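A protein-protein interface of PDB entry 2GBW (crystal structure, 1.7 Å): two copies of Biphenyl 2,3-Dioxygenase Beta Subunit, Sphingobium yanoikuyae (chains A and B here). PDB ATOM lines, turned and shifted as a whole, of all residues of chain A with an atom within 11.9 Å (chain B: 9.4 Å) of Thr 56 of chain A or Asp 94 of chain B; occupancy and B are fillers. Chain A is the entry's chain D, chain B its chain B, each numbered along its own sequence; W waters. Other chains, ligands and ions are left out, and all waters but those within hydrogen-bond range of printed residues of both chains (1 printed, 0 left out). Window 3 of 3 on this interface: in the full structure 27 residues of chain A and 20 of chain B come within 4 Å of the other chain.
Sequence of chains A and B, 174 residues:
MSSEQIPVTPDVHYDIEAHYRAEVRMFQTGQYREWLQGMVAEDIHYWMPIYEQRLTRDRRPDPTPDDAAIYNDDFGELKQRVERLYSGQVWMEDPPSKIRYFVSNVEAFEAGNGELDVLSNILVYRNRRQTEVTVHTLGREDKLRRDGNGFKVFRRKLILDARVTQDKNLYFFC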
ATOM      1  N   GLU A  52      36.660  -1.166  -8.993  1.00  0.00           N
ATOM      2  CA  GLU A  52      36.262  -2.489  -8.659  1.00  0.00           C
ATOM      3  C   GLU A  52      34.757  -2.639  -8.928  1.00  0.00           C
ATOM      4  O   GLU A  52      34.020  -1.668  -9.040  1.00  0.00           O
ATOM      5  CB  GLU A  52      36.656  -2.798  -7.225  1.00  0.00           C
ATOM      6  CG  GLU A  52      35.889  -2.100  -6.245  1.00  0.00           C
ATOM      7  CD  GLU A  52      36.344  -2.370  -4.838  1.00  0.00           C
ATOM      8  OE1 GLU A  52      36.758  -3.516  -4.535  1.00  0.00           O
ATOM      9  OE2 GLU A  52      36.311  -1.419  -4.054  1.00  0.00           O
ATOM     10  N   GLN A  53      34.319  -3.878  -9.020  1.00  0.00           N
ATOM     11  CA  GLN A  53      32.907  -4.197  -9.128  1.00  0.00           C
ATOM     12  C   GLN A  53      32.292  -4.208  -7.723  1.00  0.00           C
ATOM     13  O   GLN A  53      32.726  -4.950  -6.888  1.00  0.00           O
ATOM     14  CB  GLN A  53      32.724  -5.571  -9.770  1.00  0.00           C
ATOM     15  CG  GLN A  53      33.221  -5.690 -11.230  1.00  0.00           C
ATOM     16  CD  GLN A  53      32.382  -4.930 -12.235  1.00  0.00           C
ATOM     17  OE1 GLN A  53      31.746  -3.915 -11.915  1.00  0.00           O
ATOM     18  NE2 GLN A  53      32.403  -5.380 -13.469  1.00  0.00           N
ATOM     19  N   ARG A  54      31.311  -3.339  -7.502  1.00  0.00           N
ATOM     20  CA  ARG A  54      30.685  -3.158  -6.217  1.00  0.00           C
ATOM     21  C   ARG A  54      29.180  -3.303  -6.364  1.00  0.00           C
ATOM     22  O   ARG A  54      28.615  -2.914  -7.394  1.00  0.00           O
ATOM     23  CB  ARG A  54      30.959  -1.740  -5.710  1.00  0.00           C
ATOM     24  CG  ARG A  54      32.361  -1.471  -5.352  1.00  0.00           C
ATOM     25  CD  ARG A  54      32.522  -0.015  -4.914  1.00  0.00           C
ATOM     26  NE  ARG A  54      33.881   0.270  -4.494  1.00  0.00           N
ATOM     27  CZ  ARG A  54      34.303   1.487  -4.193  1.00  0.00           C
ATOM     28  NH1 ARG A  54      33.465   2.500  -4.269  1.00  0.00           N
ATOM     29  NH2 ARG A  54      35.554   1.691  -3.803  1.00  0.00           N
ATOM     30  N   LEU A  55      28.532  -3.764  -5.301  1.00  0.00           N
ATOM     31  CA  LEU A  55      27.063  -3.731  -5.215  1.00  0.00           C
ATOM     32  C   LEU A  55      26.526  -2.310  -5.317  1.00  0.00           C
ATOM     33  O   LEU A  55      27.151  -1.368  -4.846  1.00  0.00           O
ATOM     34  CB  LEU A  55      26.605  -4.354  -3.899  1.00  0.00           C
ATOM     35  CG  LEU A  55      26.946  -5.838  -3.784  1.00  0.00           C
ATOM     36  CD1 LEU A  55      26.599  -6.434  -2.449  1.00  0.00           C
ATOM     37  CD2 LEU A  55      26.215  -6.556  -4.884  1.00  0.00           C
ATOM     38  N   THR A  56      25.376  -2.155  -5.962  1.00  0.00           N
ATOM     39  CA  THR A  56      24.763  -0.857  -6.144  1.00  0.00           C
ATOM     40  C   THR A  56      24.460  -0.221  -4.768  1.00  0.00           C
ATOM     41  O   THR A  56      24.489   1.011  -4.634  1.00  0.00           O
ATOM     42  CB  THR A  56      23.476  -0.974  -7.046  1.00  0.00           C
ATOM     43  OG1 THR A  56      23.869  -1.052  -8.426  1.00  0.00           O
ATOM     44  CG2 THR A  56      22.539   0.227  -6.887  1.00  0.00           C
ATOM     45  N   ARG A  57      24.219  -1.051  -3.751  1.00  0.00           N
ATOM     46  CA  ARG A  57      23.909  -0.541  -2.396  1.00  0.00           C
ATOM     47  C   ARG A  57      25.143   0.024  -1.690  1.00  0.00           C
ATOM     48  O   ARG A  57      25.024   0.684  -0.648  1.00  0.00           O
ATOM     49  CB  ARG A  57      23.265  -1.630  -1.521  1.00  0.00           C
ATOM     50  CG  ARG A  57      24.197  -2.753  -1.044  1.00  0.00           C
ATOM     51  CD  ARG A  57      23.506  -3.577   0.067  1.00  0.00           C
ATOM     52  NE  ARG A  57      24.463  -4.386   0.825  1.00  0.00           N
ATOM     53  CZ  ARG A  57      24.568  -5.705   0.758  1.00  0.00           C
ATOM     54  NH1 ARG A  57      23.766  -6.403  -0.028  1.00  0.00           N
ATOM     55  NH2 ARG A  57      25.494  -6.324   1.493  1.00  0.00           N
ATOM     56  N   ASP A  58      26.323  -0.238  -2.246  1.00  0.00           N
ATOM     57  CA  ASP A  58      27.581   0.195  -1.661  1.00  0.00           C
ATOM     58  C   ASP A  58      27.742   1.695  -1.817  1.00  0.00           C
ATOM     59  O   ASP A  58      27.771   2.209  -2.922  1.00  0.00           O
ATOM     60  CB  ASP A  58      28.724  -0.491  -2.374  1.00  0.00           C
ATOM     61  CG  ASP A  58      30.019  -0.352  -1.646  1.00  0.00           C
ATOM     62  OD1 ASP A  58      30.461   0.783  -1.431  1.00  0.00           O
ATOM     63  OD2 ASP A  58      30.598  -1.399  -1.282  1.00  0.00           O
ATOM     64  N   ARG A  59      27.896   2.397  -0.711  1.00  0.00           N
ATOM     65  CA  ARG A  59      27.942   3.849  -0.781  1.00  0.00           C
ATOM     66  C   ARG A  59      29.378   4.408  -0.805  1.00  0.00           C
ATOM     67  O   ARG A  59      29.565   5.626  -0.773  1.00  0.00           O
ATOM     68  CB  ARG A  59      27.110   4.434   0.372  1.00  0.00           C
ATOM     69  CG  ARG A  59      25.591   4.169   0.234  1.00  0.00           C
ATOM     70  CD  ARG A  59      24.739   5.312   0.827  1.00  0.00           C
ATOM     71  NE  ARG A  59      24.317   5.069   2.216  1.00  0.00           N
ATOM     72  CZ  ARG A  59      25.021   5.366   3.317  1.00  0.00           C
ATOM     73  NH1 ARG A  59      26.239   5.912   3.241  1.00  0.00           N
ATOM     74  NH2 ARG A  59      24.497   5.102   4.514  1.00  0.00           N
ATOM     75  N   ARG A  60      30.396   3.551  -0.894  1.00  0.00           N
ATOM     76  CA  ARG A  60      31.771   4.053  -0.926  1.00  0.00           C
ATOM     77  C   ARG A  60      32.031   4.992  -2.109  1.00  0.00           C
ATOM     78  O   ARG A  60      31.410   4.904  -3.191  1.00  0.00           O
ATOM     79  CB  ARG A  60      32.821   2.935  -0.882  1.00  0.00           C
ATOM     80  CG  ARG A  60      32.983   2.240   0.487  1.00  0.00           C
ATOM     81  CD  ARG A  60      33.869   1.019   0.362  1.00  0.00           C
ATOM     82  NE  ARG A  60      33.259   0.007  -0.496  1.00  0.00           N
ATOM     83  CZ  ARG A  60      33.913  -1.008  -1.044  1.00  0.00           C
ATOM     84  NH1 ARG A  60      35.223  -1.140  -0.875  1.00  0.00           N
ATOM     85  NH2 ARG A  60      33.272  -1.881  -1.803  1.00  0.00           N
ATOM     86  N   PRO A  61      32.956   5.935  -1.909  1.00  0.00           N
ATOM     87  CA  PRO A  61      33.227   6.855  -3.012  1.00  0.00           C
ATOM     88  C   PRO A  61      34.042   6.173  -4.084  1.00  0.00           C
ATOM     89  O   PRO A  61      34.752   5.187  -3.801  1.00  0.00           O
ATOM     90  CB  PRO A  61      34.059   7.953  -2.364  1.00  0.00           C
ATOM     91  CG  PRO A  61      34.742   7.292  -1.231  1.00  0.00           C
ATOM     92  CD  PRO A  61      33.776   6.237  -0.717  1.00  0.00           C
ATOM     93  N   ASP A  62      33.884   6.681  -5.298  1.00  0.00           N
ATOM     94  CA  ASP A  62      34.750   6.414  -6.460  1.00  0.00           C
ATOM     95  C   ASP A  62      36.246   6.652  -6.165  1.00  0.00           C
ATOM     96  O   ASP A  62      36.607   7.457  -5.317  1.00  0.00           O
ATOM     97  CB  ASP A  62      34.350   7.313  -7.639  1.00  0.00           C
ATOM     98  CG  ASP A  62      33.319   6.677  -8.592  1.00  0.00           C
ATOM     99  OD1 ASP A  62      32.352   5.997  -8.160  1.00  0.00           O
ATOM    100  OD2 ASP A  62      33.469   6.900  -9.815  1.00  0.00           O
ATOM    101  N   ARG B  84      12.402  -1.049 -16.841  1.00  0.00           N
ATOM    102  CA  ARG B  84      13.106  -2.245 -16.372  1.00  0.00           C
ATOM    103  C   ARG B  84      14.467  -1.844 -15.816  1.00  0.00           C
ATOM    104  O   ARG B  84      14.940  -2.412 -14.826  1.00  0.00           O
ATOM    105  CB  ARG B  84      13.312  -3.260 -17.499  1.00  0.00           C
ATOM    106  CG  ARG B  84      14.055  -4.552 -17.064  1.00  0.00           C
ATOM    107  CD  ARG B  84      14.228  -5.527 -18.210  1.00  0.00           C
ATOM    108  NE  ARG B  84      15.149  -6.607 -17.834  1.00  0.00           N
ATOM    109  CZ  ARG B  84      16.459  -6.654 -18.090  1.00  0.00           C
ATOM    110  NH1 ARG B  84      17.064  -5.690 -18.766  1.00  0.00           N
ATOM    111  NH2 ARG B  84      17.191  -7.687 -17.665  1.00  0.00           N
ATOM    112  N   LEU B  85      15.096  -0.835 -16.418  1.00  0.00           N
ATOM    113  CA  LEU B  85      16.396  -0.424 -15.928  1.00  0.00           C
ATOM    114  C   LEU B  85      16.291   0.587 -14.750  1.00  0.00           C
ATOM    115  O   LEU B  85      17.321   1.014 -14.237  1.00  0.00           O
ATOM    116  CB  LEU B  85      17.261   0.085 -17.080  1.00  0.00           C
ATOM    117  CG  LEU B  85      17.360  -0.836 -18.306  1.00  0.00           C
ATOM    118  CD1 LEU B  85      17.667  -0.013 -19.562  1.00  0.00           C
ATOM    119  CD2 LEU B  85      18.395  -1.958 -18.103  1.00  0.00           C
ATOM    120  N   TYR B  86      15.060   0.922 -14.323  1.00  0.00           N
ATOM    121  CA  TYR B  86      14.769   1.853 -13.200  1.00  0.00           C
ATOM    122  C   TYR B  86      13.906   1.223 -12.115  1.00  0.00           C
ATOM    123  O   TYR B  86      14.323   1.064 -10.960  1.00  0.00           O
ATOM    124  CB  TYR B  86      13.958   3.056 -13.661  1.00  0.00           C
ATOM    125  CG  TYR B  86      14.722   4.053 -14.434  1.00  0.00           C
ATOM    126  CD1 TYR B  86      14.904   3.888 -15.789  1.00  0.00           C
ATOM    127  CD2 TYR B  86      15.257   5.182 -13.819  1.00  0.00           C
ATOM    128  CE1 TYR B  86      15.581   4.792 -16.511  1.00  0.00           C
ATOM    129  CE2 TYR B  86      15.961   6.091 -14.548  1.00  0.00           C
ATOM    130  CZ  TYR B  86      16.123   5.883 -15.897  1.00  0.00           C
ATOM    131  OH  TYR B  86      16.817   6.777 -16.650  1.00  0.00           O
ATOM    132  N   GLY B  88      13.025  -1.528 -11.388  1.00  0.00           N
ATOM    133  CA  GLY B  88      13.391  -2.844 -10.952  1.00  0.00           C
ATOM    134  C   GLY B  88      14.785  -2.953 -10.401  1.00  0.00           C
ATOM    135  O   GLY B  88      15.730  -2.359 -10.951  1.00  0.00           O
ATOM    136  N   GLN B  89      14.884  -3.664  -9.282  1.00  0.00           N
ATOM    137  CA  GLN B  89      16.111  -4.332  -8.875  1.00  0.00           C
ATOM    138  C   GLN B  89      16.232  -5.547  -9.825  1.00  0.00           C
ATOM    139  O   GLN B  89      15.560  -6.566  -9.626  1.00  0.00           O
ATOM    140  CB  GLN B  89      16.104  -4.854  -7.408  1.00  0.00           C
ATOM    141  CG  GLN B  89      14.849  -4.570  -6.492  1.00  0.00           C
ATOM    142  CD  GLN B  89      13.667  -5.538  -6.723  1.00  0.00           C
ATOM    143  OE1 GLN B  89      12.532  -5.276  -6.289  1.00  0.00           O
ATOM    144  NE2 GLN B  89      13.936  -6.662  -7.398  1.00  0.00           N
ATOM    145  N   VAL B  90      17.072  -5.403 -10.843  1.00  0.00           N
ATOM    146  CA  VAL B  90      17.418  -6.473 -11.755  1.00  0.00           C
ATOM    147  C   VAL B  90      18.816  -6.949 -11.379  1.00  0.00           C
ATOM    148  O   VAL B  90      19.793  -6.237 -11.562  1.00  0.00           O
ATOM    149  CB  VAL B  90      17.404  -5.968 -13.251  1.00  0.00           C
ATOM    150  CG1 VAL B  90      18.096  -6.949 -14.127  1.00  0.00           C
ATOM    151  CG2 VAL B  90      15.956  -5.772 -13.718  1.00  0.00           C
ATOM    152  N   TRP B  91      18.932  -8.179 -10.890  1.00  0.00           N
ATOM    153  CA  TRP B  91      20.167  -8.571 -10.238  1.00  0.00           C
ATOM    154  C   TRP B  91      21.338  -8.734 -11.193  1.00  0.00           C
ATOM    155  O   TRP B  91      22.497  -8.511 -10.803  1.00  0.00           O
ATOM    156  CB  TRP B  91      19.937  -9.836  -9.404  1.00  0.00           C
ATOM    157  CG  TRP B  91      18.860  -9.625  -8.359  1.00  0.00           C
ATOM    158  CD1 TRP B  91      17.634 -10.201  -8.320  1.00  0.00           C
ATOM    159  CD2 TRP B  91      18.910  -8.700  -7.266  1.00  0.00           C
ATOM    160  NE1 TRP B  91      16.917  -9.725  -7.230  1.00  0.00           N
ATOM    161  CE2 TRP B  91      17.683  -8.805  -6.567  1.00  0.00           C
ATOM    162  CE3 TRP B  91      19.885  -7.809  -6.792  1.00  0.00           C
ATOM    163  CZ2 TRP B  91      17.403  -8.050  -5.417  1.00  0.00           C
ATOM    164  CZ3 TRP B  91      19.618  -7.058  -5.638  1.00  0.00           C
ATOM    165  CH2 TRP B  91      18.380  -7.187  -4.968  1.00  0.00           C
ATOM    166  N   MET B  92      21.078  -9.136 -12.437  1.00  0.00           N
ATOM    167  CA  MET B  92      22.150  -9.140 -13.452  1.00  0.00           C
ATOM    168  C   MET B  92      22.778  -7.779 -13.674  1.00  0.00           C
ATOM    169  O   MET B  92      23.926  -7.718 -14.081  1.00  0.00           O
ATOM    170  CB  MET B  92      21.648  -9.602 -14.831  1.00  0.00           C
ATOM    171  CG  MET B  92      21.771 -11.040 -15.051  1.00  0.00           C
ATOM    172  SD  MET B  92      21.374 -11.418 -16.768  1.00  0.00           S
ATOM    173  CE  MET B  92      22.791 -10.771 -17.657  1.00  0.00           C
ATOM    174  N   GLU B  93      22.010  -6.702 -13.466  1.00  0.00           N
ATOM    175  CA  GLU B  93      22.481  -5.335 -13.591  1.00  0.00           C
ATOM    176  C   GLU B  93      22.825  -4.703 -12.274  1.00  0.00           C
ATOM    177  O   GLU B  93      22.759  -3.474 -12.139  1.00  0.00           O
ATOM    178  CB  GLU B  93      21.431  -4.476 -14.260  1.00  0.00           C
ATOM    179  CG  GLU B  93      21.321  -4.719 -15.700  1.00  0.00           C
ATOM    180  CD  GLU B  93      22.565  -4.252 -16.427  1.00  0.00           C
ATOM    181  OE1 GLU B  93      22.822  -3.017 -16.492  1.00  0.00           O
ATOM    182  OE2 GLU B  93      23.275  -5.151 -16.914  1.00  0.00           O
ATOM    183  N   ASP B  94      23.204  -5.522 -11.302  1.00  0.00           N
ATOM    184  CA  ASP B  94      23.722  -4.988 -10.061  1.00  0.00           C
ATOM    185  C   ASP B  94      25.202  -5.381  -9.961  1.00  0.00           C
ATOM    186  O   ASP B  94      25.513  -6.513  -9.592  1.00  0.00           O
ATOM    187  CB  ASP B  94      22.892  -5.472  -8.883  1.00  0.00           C
ATOM    188  CG  ASP B  94      23.303  -4.832  -7.566  1.00  0.00           C
ATOM    189  OD1 ASP B  94      24.063  -3.852  -7.609  1.00  0.00           O
ATOM    190  OD2 ASP B  94      22.895  -5.350  -6.484  1.00  0.00           O
ATOM    191  N   PRO B  95      26.124  -4.438 -10.277  1.00  0.00           N
ATOM    192  CA  PRO B  95      25.913  -3.064 -10.741  1.00  0.00           C
ATOM    193  C   PRO B  95      25.678  -3.037 -12.230  1.00  0.00           C
ATOM    194  O   PRO B  95      25.820  -4.042 -12.874  1.00  0.00           O
ATOM    195  CB  PRO B  95      27.228  -2.378 -10.412  1.00  0.00           C
ATOM    196  CG  PRO B  95      28.244  -3.531 -10.574  1.00  0.00           C
ATOM    197  CD  PRO B  95      27.550  -4.748 -10.097  1.00  0.00           C
ATOM    198  N   PRO B  96      25.259  -1.894 -12.771  1.00  0.00           N
ATOM    199  CA  PRO B  96      24.989  -1.953 -14.200  1.00  0.00           C
ATOM    200  C   PRO B  96      26.224  -2.385 -15.033  1.00  0.00           C
ATOM    201  O   PRO B  96      27.375  -2.071 -14.705  1.00  0.00           O
ATOM    202  CB  PRO B  96      24.539  -0.528 -14.538  1.00  0.00           C
ATOM    203  CG  PRO B  96      24.090   0.049 -13.257  1.00  0.00           C
ATOM    204  CD  PRO B  96      24.953  -0.587 -12.194  1.00  0.00           C
ATOM    205  N   SER B  97      25.968  -3.165 -16.059  1.00  0.00           N
ATOM    206  CA  SER B  97      27.006  -3.534 -17.008  1.00  0.00           C
ATOM    207  C   SER B  97      27.418  -2.264 -17.773  1.00  0.00           C
ATOM    208  O   SER B  97      26.740  -1.216 -17.725  1.00  0.00           O
ATOM    209  CB  SER B  97      26.497  -4.593 -17.938  1.00  0.00           C
ATOM    210  OG  SER B  97      25.282  -4.229 -18.497  1.00  0.00           O
ATOM    211  N   ARG B 128      30.867  -6.916 -18.740  1.00  0.00           N
ATOM    212  CA  ARG B 128      30.256  -7.099 -17.437  1.00  0.00           C
ATOM    213  C   ARG B 128      31.053  -8.118 -16.648  1.00  0.00           C
ATOM    214  O   ARG B 128      31.938  -8.811 -17.190  1.00  0.00           O
ATOM    215  CB  ARG B 128      28.804  -7.557 -17.552  1.00  0.00           C
ATOM    216  CG  ARG B 128      28.633  -8.928 -18.194  1.00  0.00           C
ATOM    217  CD  ARG B 128      27.114  -9.279 -18.391  1.00  0.00           C
ATOM    218  NE  ARG B 128      26.369  -9.179 -17.126  1.00  0.00           N
ATOM    219  CZ  ARG B 128      26.205 -10.163 -16.276  1.00  0.00           C
ATOM    220  NH1 ARG B 128      26.715 -11.372 -16.533  1.00  0.00           N
ATOM    221  NH2 ARG B 128      25.542  -9.942 -15.148  1.00  0.00           N
ATOM    222  N   ARG B 129      30.777  -8.063 -15.357  1.00  0.00           N
ATOM    223  CA  ARG B 129      31.416  -8.925 -14.362  1.00  0.00           C
ATOM    224  C   ARG B 129      32.936  -8.851 -14.552  1.00  0.00           C
ATOM    225  O   ARG B 129      33.465  -7.736 -14.572  1.00  0.00           O
ATOM    226  CB  ARG B 129      30.819 -10.307 -14.456  1.00  0.00           C
ATOM    227  CG  ARG B 129      29.289 -10.370 -14.123  1.00  0.00           C
ATOM    228  CD  ARG B 129      28.952  -9.846 -12.724  1.00  0.00           C
ATOM    229  NE  ARG B 129      27.512 -10.122 -12.431  1.00  0.00           N
ATOM    230  CZ  ARG B 129      26.736  -9.376 -11.662  1.00  0.00           C
ATOM    231  NH1 ARG B 129      27.220  -8.277 -11.066  1.00  0.00           N
ATOM    232  NH2 ARG B 129      25.450  -9.689 -11.509  1.00  0.00           N
HETATM  233  O   HOH W   1      22.877  -3.659  -4.131  1.00  0.00           O
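The side-chain carboxylate of Asp 94 of chain B is in hydrogen-bond range of the backbone NH of Thr 56 of chain A, at 2.7 Å.
O of Arg 129 of chain B sits at hydrogen-bond distance from NE2 of Gln 53 of chain A.
The guanidinium group (NH2) of Arg 129 of chain B lies within hydrogen-bond range of the backbone carbonyl oxygen (O) of Trp 91 of chain B, at 3.3 Å.
The backbone carbonyl oxygen (O) of Pro 61 of chain A sits at hydrogen-bond distance from the guanidinium group (NH1) of Arg 54 of chain A (3.0 Å).
The guanidinium group of Arg 54 of chain A is in hydrogen-bond range of the backbone carbonyl oxygen of Arg 60 of chain A, at 3.3 Å.
O of Asp 94 of chain B lies within hydrogen-bond range of NH1 of Arg 129 of chain B, at 2.9 Å.
OE2 of Glu 52 of chain A lies within salt-bridge range of NE of Arg 54 of chain A, at 3.0 Å.
Gln 53 of chain A touches Pro 95 of chain B (OE1 to CG, 3.8 Å).
Pro 95 of chain B touches Arg 54 of chain A (CG to O, 3.3 Å).
Asp 94 of chain B touches Leu 55 of chain A (OD1 to C, 3.7 Å).
OG1 of Thr 56 of chain A touches CA of Pro 95 of chain B, at 3.7 Å.
OG1 of Thr 56 of chain A touches CD of Pro 96 of chain B, 3.9 Å away.
Printed residues of chain B within 4 Å of Gln 53 of chain A: Pro 95 (3.8 Å) and Arg 129 (2.8 Å).
Printed residues of chain B within 4 Å of Arg 54 of chain A: Pro 95 (3.3 Å).
Printed residues of chain B within 4 Å of Leu 55 of chain A: Asp 94.
Thr 56 of chain A touches just these residues of chain B: Asp 94, Pro 95 and Pro 96.
No residue of chain A comes within 4 Å of Glu 93 of chain B.
Asp 94 of chain B touches two residues of chain A.
Of the printed residues of chain A, Pro 95 of chain B touches Gln 53, Arg 54 and Thr 56.
Pro 96 of chain B touches just one residue of chain A: Thr 56.
Ser 97 of chain B touches none of the printed residues of chain A.
Printed residues of chain A within 4 Å of Arg 129 of chain B: Gln 53 (2.8 Å).
The nearest residue of chain B that does not touch Thr 56 of chain A is Glu 93 of chain B (4.6 Å).
The nearest printed residue of chain B that does not touch Gln 53 of chain A is Arg 128 of chain B (4.4 Å).
Printed residues of chain B that touch a printed residue of chain A: Asp 94, Pro 95, Pro 96 and Arg 129.
Among the printed residues, no Asp or Glu carboxylate lies within 4 Å of a Lys or Arg side-chain nitrogen of the other chain.
No position is printed for both chains.
Water W1 lies within hydrogen-bond range of OD2 of Asp 94 of chain B (2.9 Å), N of Arg 57 of chain A (3.0 Å) and N of Thr 56 of chain A (3.4 Å).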
